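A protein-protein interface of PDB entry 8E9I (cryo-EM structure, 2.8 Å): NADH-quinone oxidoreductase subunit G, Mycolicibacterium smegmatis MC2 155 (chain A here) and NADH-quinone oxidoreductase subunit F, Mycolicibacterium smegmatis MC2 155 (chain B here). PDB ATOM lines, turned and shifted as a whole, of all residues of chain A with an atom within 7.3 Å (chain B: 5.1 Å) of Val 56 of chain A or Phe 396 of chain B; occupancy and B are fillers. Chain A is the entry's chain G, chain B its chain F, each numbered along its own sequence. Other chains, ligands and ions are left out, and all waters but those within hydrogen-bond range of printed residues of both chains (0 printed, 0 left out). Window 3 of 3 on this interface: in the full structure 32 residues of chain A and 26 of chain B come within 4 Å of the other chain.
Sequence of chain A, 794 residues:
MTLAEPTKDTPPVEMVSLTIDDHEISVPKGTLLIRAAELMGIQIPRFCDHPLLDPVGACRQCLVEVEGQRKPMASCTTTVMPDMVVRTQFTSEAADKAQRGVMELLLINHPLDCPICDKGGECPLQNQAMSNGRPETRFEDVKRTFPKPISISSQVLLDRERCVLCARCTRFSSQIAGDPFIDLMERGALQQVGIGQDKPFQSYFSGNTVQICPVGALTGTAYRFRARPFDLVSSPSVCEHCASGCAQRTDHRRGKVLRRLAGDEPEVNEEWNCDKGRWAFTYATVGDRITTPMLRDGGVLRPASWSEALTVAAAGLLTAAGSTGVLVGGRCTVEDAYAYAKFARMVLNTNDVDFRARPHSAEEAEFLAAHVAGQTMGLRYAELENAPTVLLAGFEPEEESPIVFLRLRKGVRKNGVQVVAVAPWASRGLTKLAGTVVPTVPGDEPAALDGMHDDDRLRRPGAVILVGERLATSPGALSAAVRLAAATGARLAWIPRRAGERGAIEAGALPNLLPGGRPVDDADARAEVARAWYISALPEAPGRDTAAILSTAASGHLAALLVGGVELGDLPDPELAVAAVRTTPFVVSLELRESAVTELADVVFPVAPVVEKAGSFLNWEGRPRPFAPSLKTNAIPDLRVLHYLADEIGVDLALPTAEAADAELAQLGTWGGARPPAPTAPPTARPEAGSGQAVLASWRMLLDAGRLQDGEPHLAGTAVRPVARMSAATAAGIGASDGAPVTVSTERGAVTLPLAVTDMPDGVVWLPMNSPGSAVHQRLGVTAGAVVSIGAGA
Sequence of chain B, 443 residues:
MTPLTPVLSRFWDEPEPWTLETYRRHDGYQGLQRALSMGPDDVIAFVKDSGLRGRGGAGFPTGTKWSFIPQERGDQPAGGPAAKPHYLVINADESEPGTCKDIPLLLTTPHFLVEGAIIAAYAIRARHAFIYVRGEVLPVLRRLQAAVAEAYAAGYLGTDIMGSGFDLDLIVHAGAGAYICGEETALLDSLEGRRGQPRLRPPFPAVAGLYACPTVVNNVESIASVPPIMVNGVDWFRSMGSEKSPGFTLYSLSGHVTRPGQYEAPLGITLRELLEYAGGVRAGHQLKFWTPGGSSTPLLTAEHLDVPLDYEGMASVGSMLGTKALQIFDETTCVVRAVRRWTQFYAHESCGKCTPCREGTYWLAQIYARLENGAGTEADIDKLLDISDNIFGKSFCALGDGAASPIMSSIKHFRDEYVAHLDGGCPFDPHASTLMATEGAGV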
ATOM      1  N   CYS A  48      -7.241  19.752  -0.845  1.00  0.00           N
ATOM      2  CA  CYS A  48      -7.305  21.203  -0.916  1.00  0.00           C
ATOM      3  C   CYS A  48      -6.839  21.729  -2.258  1.00  0.00           C
ATOM      4  O   CYS A  48      -7.261  22.816  -2.661  1.00  0.00           O
ATOM      5  CB  CYS A  48      -6.478  21.824   0.206  1.00  0.00           C
ATOM      6  SG  CYS A  48      -4.709  21.836  -0.072  1.00  0.00           S
ATOM      7  N   ASP A  49      -6.000  20.985  -2.965  1.00  0.00           N
ATOM      8  CA  ASP A  49      -5.537  21.435  -4.264  1.00  0.00           C
ATOM      9  C   ASP A  49      -6.704  21.614  -5.219  1.00  0.00           C
ATOM     10  O   ASP A  49      -7.702  20.897  -5.145  1.00  0.00           O
ATOM     11  CB  ASP A  49      -4.557  20.436  -4.855  1.00  0.00           C
ATOM     12  CG  ASP A  49      -4.179  20.782  -6.268  1.00  0.00           C
ATOM     13  OD1 ASP A  49      -4.005  21.982  -6.551  1.00  0.00           O
ATOM     14  OD2 ASP A  49      -4.082  19.867  -7.107  1.00  0.00           O
ATOM     15  N   HIS A  50      -6.573  22.582  -6.119  1.00  0.00           N
ATOM     16  CA  HIS A  50      -7.507  22.719  -7.197  1.00  0.00           C
ATOM     17  C   HIS A  50      -6.764  23.418  -8.326  1.00  0.00           C
ATOM     18  O   HIS A  50      -6.118  24.447  -8.078  1.00  0.00           O
ATOM     19  CB  HIS A  50      -8.747  23.511  -6.811  1.00  0.00           C
ATOM     20  CG  HIS A  50      -9.865  23.380  -7.794  1.00  0.00           C
ATOM     21  ND1 HIS A  50      -9.977  24.187  -8.904  1.00  0.00           N
ATOM     22  CD2 HIS A  50     -10.904  22.520  -7.849  1.00  0.00           C
ATOM     23  CE1 HIS A  50     -11.047  23.836  -9.594  1.00  0.00           C
ATOM     24  NE2 HIS A  50     -11.626  22.825  -8.976  1.00  0.00           N
ATOM     25  N   LEU A  53      -7.811  27.061  -8.607  1.00  0.00           N
ATOM     26  CA  LEU A  53      -7.691  27.886  -7.414  1.00  0.00           C
ATOM     27  C   LEU A  53      -6.222  28.094  -7.075  1.00  0.00           C
ATOM     28  O   LEU A  53      -5.387  27.213  -7.291  1.00  0.00           O
ATOM     29  CB  LEU A  53      -8.395  27.251  -6.216  1.00  0.00           C
ATOM     30  CG  LEU A  53      -9.887  26.969  -6.353  1.00  0.00           C
ATOM     31  CD1 LEU A  53     -10.428  26.424  -5.054  1.00  0.00           C
ATOM     32  CD2 LEU A  53     -10.627  28.218  -6.747  1.00  0.00           C
ATOM     33  N   ASP A  54      -5.913  29.262  -6.535  1.00  0.00           N
ATOM     34  CA  ASP A  54      -4.551  29.525  -6.109  1.00  0.00           C
ATOM     35  C   ASP A  54      -4.163  28.504  -5.048  1.00  0.00           C
ATOM     36  O   ASP A  54      -4.944  28.262  -4.117  1.00  0.00           O
ATOM     37  CB  ASP A  54      -4.424  30.940  -5.555  1.00  0.00           C
ATOM     38  N   PRO A  55      -2.996  27.874  -5.149  1.00  0.00           N
ATOM     39  CA  PRO A  55      -2.662  26.815  -4.197  1.00  0.00           C
ATOM     40  C   PRO A  55      -2.643  27.332  -2.774  1.00  0.00           C
ATOM     41  O   PRO A  55      -2.219  28.455  -2.500  1.00  0.00           O
ATOM     42  CB  PRO A  55      -1.269  26.359  -4.644  1.00  0.00           C
ATOM     43  CG  PRO A  55      -0.721  27.499  -5.392  1.00  0.00           C
ATOM     44  CD  PRO A  55      -1.882  28.146  -6.068  1.00  0.00           C
ATOM     45  N   VAL A  56      -3.126  26.493  -1.862  1.00  0.00           N
ATOM     46  CA  VAL A  56      -3.138  26.832  -0.443  1.00  0.00           C
ATOM     47  C   VAL A  56      -2.388  25.830   0.411  1.00  0.00           C
ATOM     48  O   VAL A  56      -1.970  26.172   1.529  1.00  0.00           O
ATOM     49  CB  VAL A  56      -4.592  26.985   0.059  1.00  0.00           C
ATOM     50  CG1 VAL A  56      -5.302  25.648   0.074  1.00  0.00           C
ATOM     51  CG2 VAL A  56      -4.617  27.613   1.427  1.00  0.00           C
ATOM     52  N   GLY A  57      -2.176  24.599  -0.048  1.00  0.00           N
ATOM     53  CA  GLY A  57      -1.418  23.634   0.721  1.00  0.00           C
ATOM     54  C   GLY A  57      -1.943  23.386   2.112  1.00  0.00           C
ATOM     55  O   GLY A  57      -1.159  23.065   3.007  1.00  0.00           O
ATOM     56  N   ALA A  58      -3.250  23.521   2.321  1.00  0.00           N
ATOM     57  CA  ALA A  58      -3.800  23.455   3.668  1.00  0.00           C
ATOM     58  C   ALA A  58      -3.856  22.022   4.171  1.00  0.00           C
ATOM     59  O   ALA A  58      -3.261  21.688   5.199  1.00  0.00           O
ATOM     60  CB  ALA A  58      -5.191  24.083   3.694  1.00  0.00           C
ATOM     61  N   CYS A  59      -4.560  21.152   3.453  1.00  0.00           N
ATOM     62  CA  CYS A  59      -4.852  19.830   3.980  1.00  0.00           C
ATOM     63  C   CYS A  59      -3.613  18.966   4.144  1.00  0.00           C
ATOM     64  O   CYS A  59      -3.672  17.970   4.869  1.00  0.00           O
ATOM     65  CB  CYS A  59      -5.858  19.121   3.078  1.00  0.00           C
ATOM     66  SG  CYS A  59      -5.145  18.408   1.599  1.00  0.00           S
ATOM     67  N   ARG A  60      -2.503  19.307   3.497  1.00  0.00           N
ATOM     68  CA  ARG A  60      -1.270  18.532   3.583  1.00  0.00           C
ATOM     69  C   ARG A  60      -1.453  17.095   3.120  1.00  0.00           C
ATOM     70  O   ARG A  60      -0.689  16.215   3.516  1.00  0.00           O
ATOM     71  CB  ARG A  60      -0.708  18.529   5.007  1.00  0.00           C
ATOM     72  CG  ARG A  60      -0.616  19.882   5.665  1.00  0.00           C
ATOM     73  CD  ARG A  60       0.193  20.853   4.846  1.00  0.00           C
ATOM     74  NE  ARG A  60       1.592  20.468   4.766  1.00  0.00           N
ATOM     75  CZ  ARG A  60       2.487  21.086   4.011  1.00  0.00           C
ATOM     76  NH1 ARG A  60       2.163  22.130   3.272  1.00  0.00           N
ATOM     77  NH2 ARG A  60       3.738  20.640   3.992  1.00  0.00           N
ATOM     78  N   LYS A  71      11.903  18.030   5.072  1.00  0.00           N
ATOM     79  CA  LYS A  71      10.481  17.812   5.256  1.00  0.00           C
ATOM     80  C   LYS A  71       9.833  17.328   3.960  1.00  0.00           C
ATOM     81  O   LYS A  71      10.326  17.611   2.869  1.00  0.00           O
ATOM     82  CB  LYS A  71       9.803  19.101   5.703  1.00  0.00           C
ATOM     83  CG  LYS A  71      10.217  19.587   7.079  1.00  0.00           C
ATOM     84  CD  LYS A  71       9.315  20.709   7.570  1.00  0.00           C
ATOM     85  CE  LYS A  71       9.419  21.950   6.701  1.00  0.00           C
ATOM     86  NZ  LYS A  71       8.595  23.068   7.226  1.00  0.00           N
ATOM     87  N   ALA A  74       4.332  19.771   0.147  1.00  0.00           N
ATOM     88  CA  ALA A  74       3.022  19.688  -0.479  1.00  0.00           C
ATOM     89  C   ALA A  74       3.190  19.805  -1.985  1.00  0.00           C
ATOM     90  O   ALA A  74       3.508  20.880  -2.499  1.00  0.00           O
ATOM     91  CB  ALA A  74       2.115  20.787   0.058  1.00  0.00           C
ATOM     92  N   CYS A  76       1.136  20.069  -4.203  1.00  0.00           N
ATOM     93  CA  CYS A  76       0.251  21.053  -4.802  1.00  0.00           C
ATOM     94  C   CYS A  76       0.836  22.452  -4.768  1.00  0.00           C
ATOM     95  O   CYS A  76       0.384  23.313  -5.528  1.00  0.00           O
ATOM     96  CB  CYS A  76      -1.106  21.037  -4.100  1.00  0.00           C
ATOM     97  SG  CYS A  76      -1.121  21.705  -2.438  1.00  0.00           S
ATOM     98  N   THR A  77       1.822  22.705  -3.912  1.00  0.00           N
ATOM     99  CA  THR A  77       2.380  24.042  -3.771  1.00  0.00           C
ATOM    100  C   THR A  77       3.840  24.129  -4.179  1.00  0.00           C
ATOM    101  O   THR A  77       4.388  25.234  -4.227  1.00  0.00           O
ATOM    102  CB  THR A  77       2.253  24.518  -2.325  1.00  0.00           C
ATOM    103  OG1 THR A  77       3.259  23.886  -1.527  1.00  0.00           O
ATOM    104  CG2 THR A  77       0.903  24.165  -1.776  1.00  0.00           C
ATOM    105  N   LEU A 165     -12.270  20.885   5.890  1.00  0.00           N
ATOM    106  CA  LEU A 165     -11.698  22.224   6.016  1.00  0.00           C
ATOM    107  C   LEU A 165     -10.600  22.457   4.990  1.00  0.00           C
ATOM    108  O   LEU A 165      -9.551  23.021   5.295  1.00  0.00           O
ATOM    109  CB  LEU A 165     -11.176  22.469   7.429  1.00  0.00           C
ATOM    110  CG  LEU A 165     -12.267  22.610   8.482  1.00  0.00           C
ATOM    111  CD1 LEU A 165     -11.742  22.236   9.852  1.00  0.00           C
ATOM    112  CD2 LEU A 165     -12.805  24.023   8.484  1.00  0.00           C
ATOM    113  N   CYS A 166     -10.836  22.015   3.763  1.00  0.00           N
ATOM    114  CA  CYS A 166      -9.885  22.242   2.688  1.00  0.00           C
ATOM    115  C   CYS A 166      -9.890  23.679   2.199  1.00  0.00           C
ATOM    116  O   CYS A 166      -8.900  24.116   1.610  1.00  0.00           O
ATOM    117  CB  CYS A 166     -10.187  21.309   1.519  1.00  0.00           C
ATOM    118  SG  CYS A 166     -11.682  21.717   0.632  1.00  0.00           S
ATOM    119  N   ALA A 167     -10.967  24.418   2.435  1.00  0.00           N
ATOM    120  CA  ALA A 167     -11.109  25.814   2.043  1.00  0.00           C
ATOM    121  C   ALA A 167     -11.327  25.985   0.549  1.00  0.00           C
ATOM    122  O   ALA A 167     -11.253  27.108   0.044  1.00  0.00           O
ATOM    123  CB  ALA A 167      -9.895  26.640   2.480  1.00  0.00           C
ATOM    124  N   ARG A 168     -11.598  24.904  -0.181  1.00  0.00           N
ATOM    125  CA  ARG A 168     -11.864  25.047  -1.608  1.00  0.00           C
ATOM    126  C   ARG A 168     -13.139  25.830  -1.864  1.00  0.00           C
ATOM    127  O   ARG A 168     -13.196  26.631  -2.798  1.00  0.00           O
ATOM    128  CB  ARG A 168     -11.911  23.681  -2.277  1.00  0.00           C
ATOM    129  CG  ARG A 168     -10.529  23.144  -2.477  1.00  0.00           C
ATOM    130  CD  ARG A 168     -10.492  21.737  -2.977  1.00  0.00           C
ATOM    131  NE  ARG A 168     -11.156  21.562  -4.258  1.00  0.00           N
ATOM    132  CZ  ARG A 168     -11.358  20.380  -4.814  1.00  0.00           C
ATOM    133  NH1 ARG A 168     -10.829  19.287  -4.305  1.00  0.00           N
ATOM    134  NH2 ARG A 168     -12.086  20.296  -5.921  1.00  0.00           N
ATOM    135  N   ARG A 171     -12.118  29.411  -0.950  1.00  0.00           N
ATOM    136  CA  ARG A 171     -11.163  29.920  -1.918  1.00  0.00           C
ATOM    137  C   ARG A 171     -11.833  30.177  -3.259  1.00  0.00           C
ATOM    138  O   ARG A 171     -11.474  31.122  -3.964  1.00  0.00           O
ATOM    139  CB  ARG A 171     -10.004  28.940  -2.063  1.00  0.00           C
ATOM    140  CG  ARG A 171      -9.076  28.952  -0.877  1.00  0.00           C
ATOM    141  CD  ARG A 171      -8.310  27.659  -0.746  1.00  0.00           C
ATOM    142  NE  ARG A 171      -7.602  27.329  -1.975  1.00  0.00           N
ATOM    143  CZ  ARG A 171      -7.519  26.116  -2.503  1.00  0.00           C
ATOM    144  NH1 ARG A 171      -8.060  25.063  -1.914  1.00  0.00           N
ATOM    145  NH2 ARG A 171      -6.865  25.954  -3.647  1.00  0.00           N
ATOM    146  N   PRO B 198      -0.862  31.418   9.106  1.00  0.00           N
ATOM    147  CA  PRO B 198       0.365  31.558   8.322  1.00  0.00           C
ATOM    148  C   PRO B 198       0.102  31.457   6.829  1.00  0.00           C
ATOM    149  O   PRO B 198      -0.819  30.772   6.378  1.00  0.00           O
ATOM    150  CB  PRO B 198       1.227  30.391   8.810  1.00  0.00           C
ATOM    151  CG  PRO B 198       0.256  29.391   9.287  1.00  0.00           C
ATOM    152  CD  PRO B 198      -0.874  30.169   9.881  1.00  0.00           C
ATOM    153  N   ARG B 199       0.933  32.147   6.058  1.00  0.00           N
ATOM    154  CA  ARG B 199       0.857  32.090   4.610  1.00  0.00           C
ATOM    155  C   ARG B 199       1.783  31.011   4.067  1.00  0.00           C
ATOM    156  O   ARG B 199       2.508  30.341   4.804  1.00  0.00           O
ATOM    157  CB  ARG B 199       1.238  33.429   3.992  1.00  0.00           C
ATOM    158  CG  ARG B 199       0.411  34.605   4.431  1.00  0.00           C
ATOM    159  CD  ARG B 199       1.055  35.873   3.931  1.00  0.00           C
ATOM    160  NE  ARG B 199       0.435  37.069   4.483  1.00  0.00           N
ATOM    161  CZ  ARG B 199       0.775  38.303   4.147  1.00  0.00           C
ATOM    162  NH1 ARG B 199       1.730  38.541   3.266  1.00  0.00           N
ATOM    163  NH2 ARG B 199       0.139  39.325   4.709  1.00  0.00           N
ATOM    164  N   LEU B 200       1.756  30.856   2.747  1.00  0.00           N
ATOM    165  CA  LEU B 200       2.735  30.020   2.071  1.00  0.00           C
ATOM    166  C   LEU B 200       4.097  30.700   2.076  1.00  0.00           C
ATOM    167  O   LEU B 200       4.217  31.896   2.349  1.00  0.00           O
ATOM    168  CB  LEU B 200       2.304  29.746   0.635  1.00  0.00           C
ATOM    169  CG  LEU B 200       1.246  28.668   0.422  1.00  0.00           C
ATOM    170  CD1 LEU B 200       0.786  28.662  -1.019  1.00  0.00           C
ATOM    171  CD2 LEU B 200       1.794  27.309   0.799  1.00  0.00           C
ATOM    172  N   LYS B 353      -5.691  25.507  10.185  1.00  0.00           N
ATOM    173  CA  LYS B 353      -5.556  25.579   8.738  1.00  0.00           C
ATOM    174  C   LYS B 353      -5.287  24.212   8.126  1.00  0.00           C
ATOM    175  O   LYS B 353      -5.930  23.833   7.142  1.00  0.00           O
ATOM    176  CB  LYS B 353      -4.444  26.555   8.370  1.00  0.00           C
ATOM    177  CG  LYS B 353      -4.165  26.629   6.887  1.00  0.00           C
ATOM    178  CD  LYS B 353      -3.278  27.799   6.554  1.00  0.00           C
ATOM    179  CE  LYS B 353      -3.025  27.876   5.070  1.00  0.00           C
ATOM    180  NZ  LYS B 353      -2.827  29.275   4.619  1.00  0.00           N
ATOM    181  N   CYS B 354      -4.353  23.454   8.689  1.00  0.00           N
ATOM    182  CA  CYS B 354      -3.863  22.235   8.061  1.00  0.00           C
ATOM    183  C   CYS B 354      -4.303  21.008   8.844  1.00  0.00           C
ATOM    184  O   CYS B 354      -4.382  21.038  10.074  1.00  0.00           O
ATOM    185  CB  CYS B 354      -2.338  22.263   7.930  1.00  0.00           C
ATOM    186  SG  CYS B 354      -1.425  22.196   9.469  1.00  0.00           S
ATOM    187  N   LYS B 394       5.040  17.469   8.946  1.00  0.00           N
ATOM    188  CA  LYS B 394       3.948  17.474   7.982  1.00  0.00           C
ATOM    189  C   LYS B 394       3.042  18.689   8.115  1.00  0.00           C
ATOM    190  O   LYS B 394       2.397  19.079   7.136  1.00  0.00           O
ATOM    191  CB  LYS B 394       3.099  16.209   8.128  1.00  0.00           C
ATOM    192  CG  LYS B 394       3.860  14.966   8.547  1.00  0.00           C
ATOM    193  CD  LYS B 394       5.046  14.676   7.656  1.00  0.00           C
ATOM    194  CE  LYS B 394       5.658  13.342   8.014  1.00  0.00           C
ATOM    195  NZ  LYS B 394       6.296  13.373   9.355  1.00  0.00           N
ATOM    196  N   SER B 395       2.974  19.293   9.294  1.00  0.00           N
ATOM    197  CA  SER B 395       2.072  20.411   9.507  1.00  0.00           C
ATOM    198  C   SER B 395       2.528  21.628   8.708  1.00  0.00           C
ATOM    199  O   SER B 395       3.707  21.793   8.389  1.00  0.00           O
ATOM    200  CB  SER B 395       1.994  20.757  10.987  1.00  0.00           C
ATOM    201  OG  SER B 395       3.171  21.417  11.411  1.00  0.00           O
ATOM    202  N   PHE B 396       1.568  22.495   8.391  1.00  0.00           N
ATOM    203  CA  PHE B 396       1.849  23.590   7.472  1.00  0.00           C
ATOM    204  C   PHE B 396       2.910  24.526   8.028  1.00  0.00           C
ATOM    205  O   PHE B 396       3.866  24.870   7.327  1.00  0.00           O
ATOM    206  CB  PHE B 396       0.561  24.347   7.169  1.00  0.00           C
ATOM    207  CG  PHE B 396       0.726  25.446   6.174  1.00  0.00           C
ATOM    208  CD1 PHE B 396       0.671  25.181   4.823  1.00  0.00           C
ATOM    209  CD2 PHE B 396       0.925  26.743   6.587  1.00  0.00           C
ATOM    210  CE1 PHE B 396       0.819  26.190   3.908  1.00  0.00           C
ATOM    211  CE2 PHE B 396       1.072  27.754   5.677  1.00  0.00           C
ATOM    212  CZ  PHE B 396       1.019  27.479   4.335  1.00  0.00           C
ATOM    213  N   CYS B 397       2.775  24.934   9.285  1.00  0.00           N
ATOM    214  CA  CYS B 397       3.743  25.811   9.918  1.00  0.00           C
ATOM    215  C   CYS B 397       4.399  25.052  11.056  1.00  0.00           C
ATOM    216  O   CYS B 397       4.101  23.882  11.303  1.00  0.00           O
ATOM    217  CB  CYS B 397       3.100  27.094  10.448  1.00  0.00           C
ATOM    218  SG  CYS B 397       2.283  26.897  12.030  1.00  0.00           S
ATOM    219  N   ALA B 398       5.286  25.738  11.764  1.00  0.00           N
ATOM    220  CA  ALA B 398       6.036  25.092  12.828  1.00  0.00           C
ATOM    221  C   ALA B 398       5.235  24.908  14.104  1.00  0.00           C
ATOM    222  O   ALA B 398       5.754  24.293  15.034  1.00  0.00           O
ATOM    223  CB  ALA B 398       7.302  25.889  13.128  1.00  0.00           C
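Of the 20 printed residues of chain A, 5 touch a printed residue of chain B. Of the 10 printed residues of chain B, 5 touch a printed residue of chain A. Hydrophobic or aromatic side chains of chain B within 4 Å of the printed part of chain A: Leu 200 and Phe 396. Among the printed residues, no Asp or Glu carboxylate lies within 4 Å of a Lys or Arg side-chain nitrogen of the other chain.
NE of Arg 60 of chain A sits at hydrogen-bond distance from O of Lys 394 of chain B (2.9 Å).
Of the printed residues of chain B, Val 56 of chain A touches Leu 200 (3.999 Å), Lys 353 (3.98 Å) and Phe 396 (3.7 Å). Printed residues of chain B within 4 Å of Ala 58 of chain A: Lys 353 and Cys 354. Cys 59 of chain A touches none of the printed residues of chain B. Printed residues of chain B within 4 Å of Arg 60 of chain A: Cys 354 (3.7 Å), Lys 394 (2.9 Å) and Phe 396 (3.7 Å). Thr 77 of chain A touches none of the printed residues of chain B. Printed residues of chain A within 4 Å of Leu 200 of chain B: Pro 55 (3.4 Å) and Val 56 (3.999 Å). Printed residues of chain A within 4 Å of Lys 394 of chain B: Arg 60 (2.9 Å). Phe 396 of chain B touches three residues of chain A. The nearest printed residue of chain B that does not touch Val 56 of chain A is Arg 199 of chain B (6.6 Å). The nearest residue of chain A that does not touch Phe 396 of chain B is Ala 58 of chain A (4.9 Å). The nearest printed residue of chain B that does not touch Gly 57 of chain A is Leu 200 of chain B (4.9 Å).
Among the printed residues, pairs that only touch across the chains: Ala 58 of chain A with Cys 354 of chain B, Gly 57 of chain A with Phe 396 of chain B, Pro 55 of chain A with Leu 200 of chain B, Ala 58 of chain A with Lys 353 of chain B, Val 56 of chain A with Phe 396 of chain B, Arg 60 of chain A with Cys 354 of chain B, Arg 60 of chain A with Phe 396 of chain B, Val 56 of chain A with Lys 353 of chain B and Val 56 of chain A with Leu 200 of chain B.
SG of Cys 48 of chain A lies close to N of Gly 57 of chain A (3.7 Å). The guanidinium group of Arg 60 of chain A lies close to the backbone carbonyl oxygen of Gly 57 of chain A, at 3.5 Å. The side-chain amino group (NZ) of Lys 353 of chain B lies within hydrogen-bond range of the backbone carbonyl oxygen (O) of Pro 198 of chain B. SG of Cys 354 of chain B lies close to N of Phe 396 of chain B (3.2 Å). The side-chain sulfur (SG) of Cys 48 of chain A sits close to the backbone NH (N) of Ala 58 of chain A (3.3 Å).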
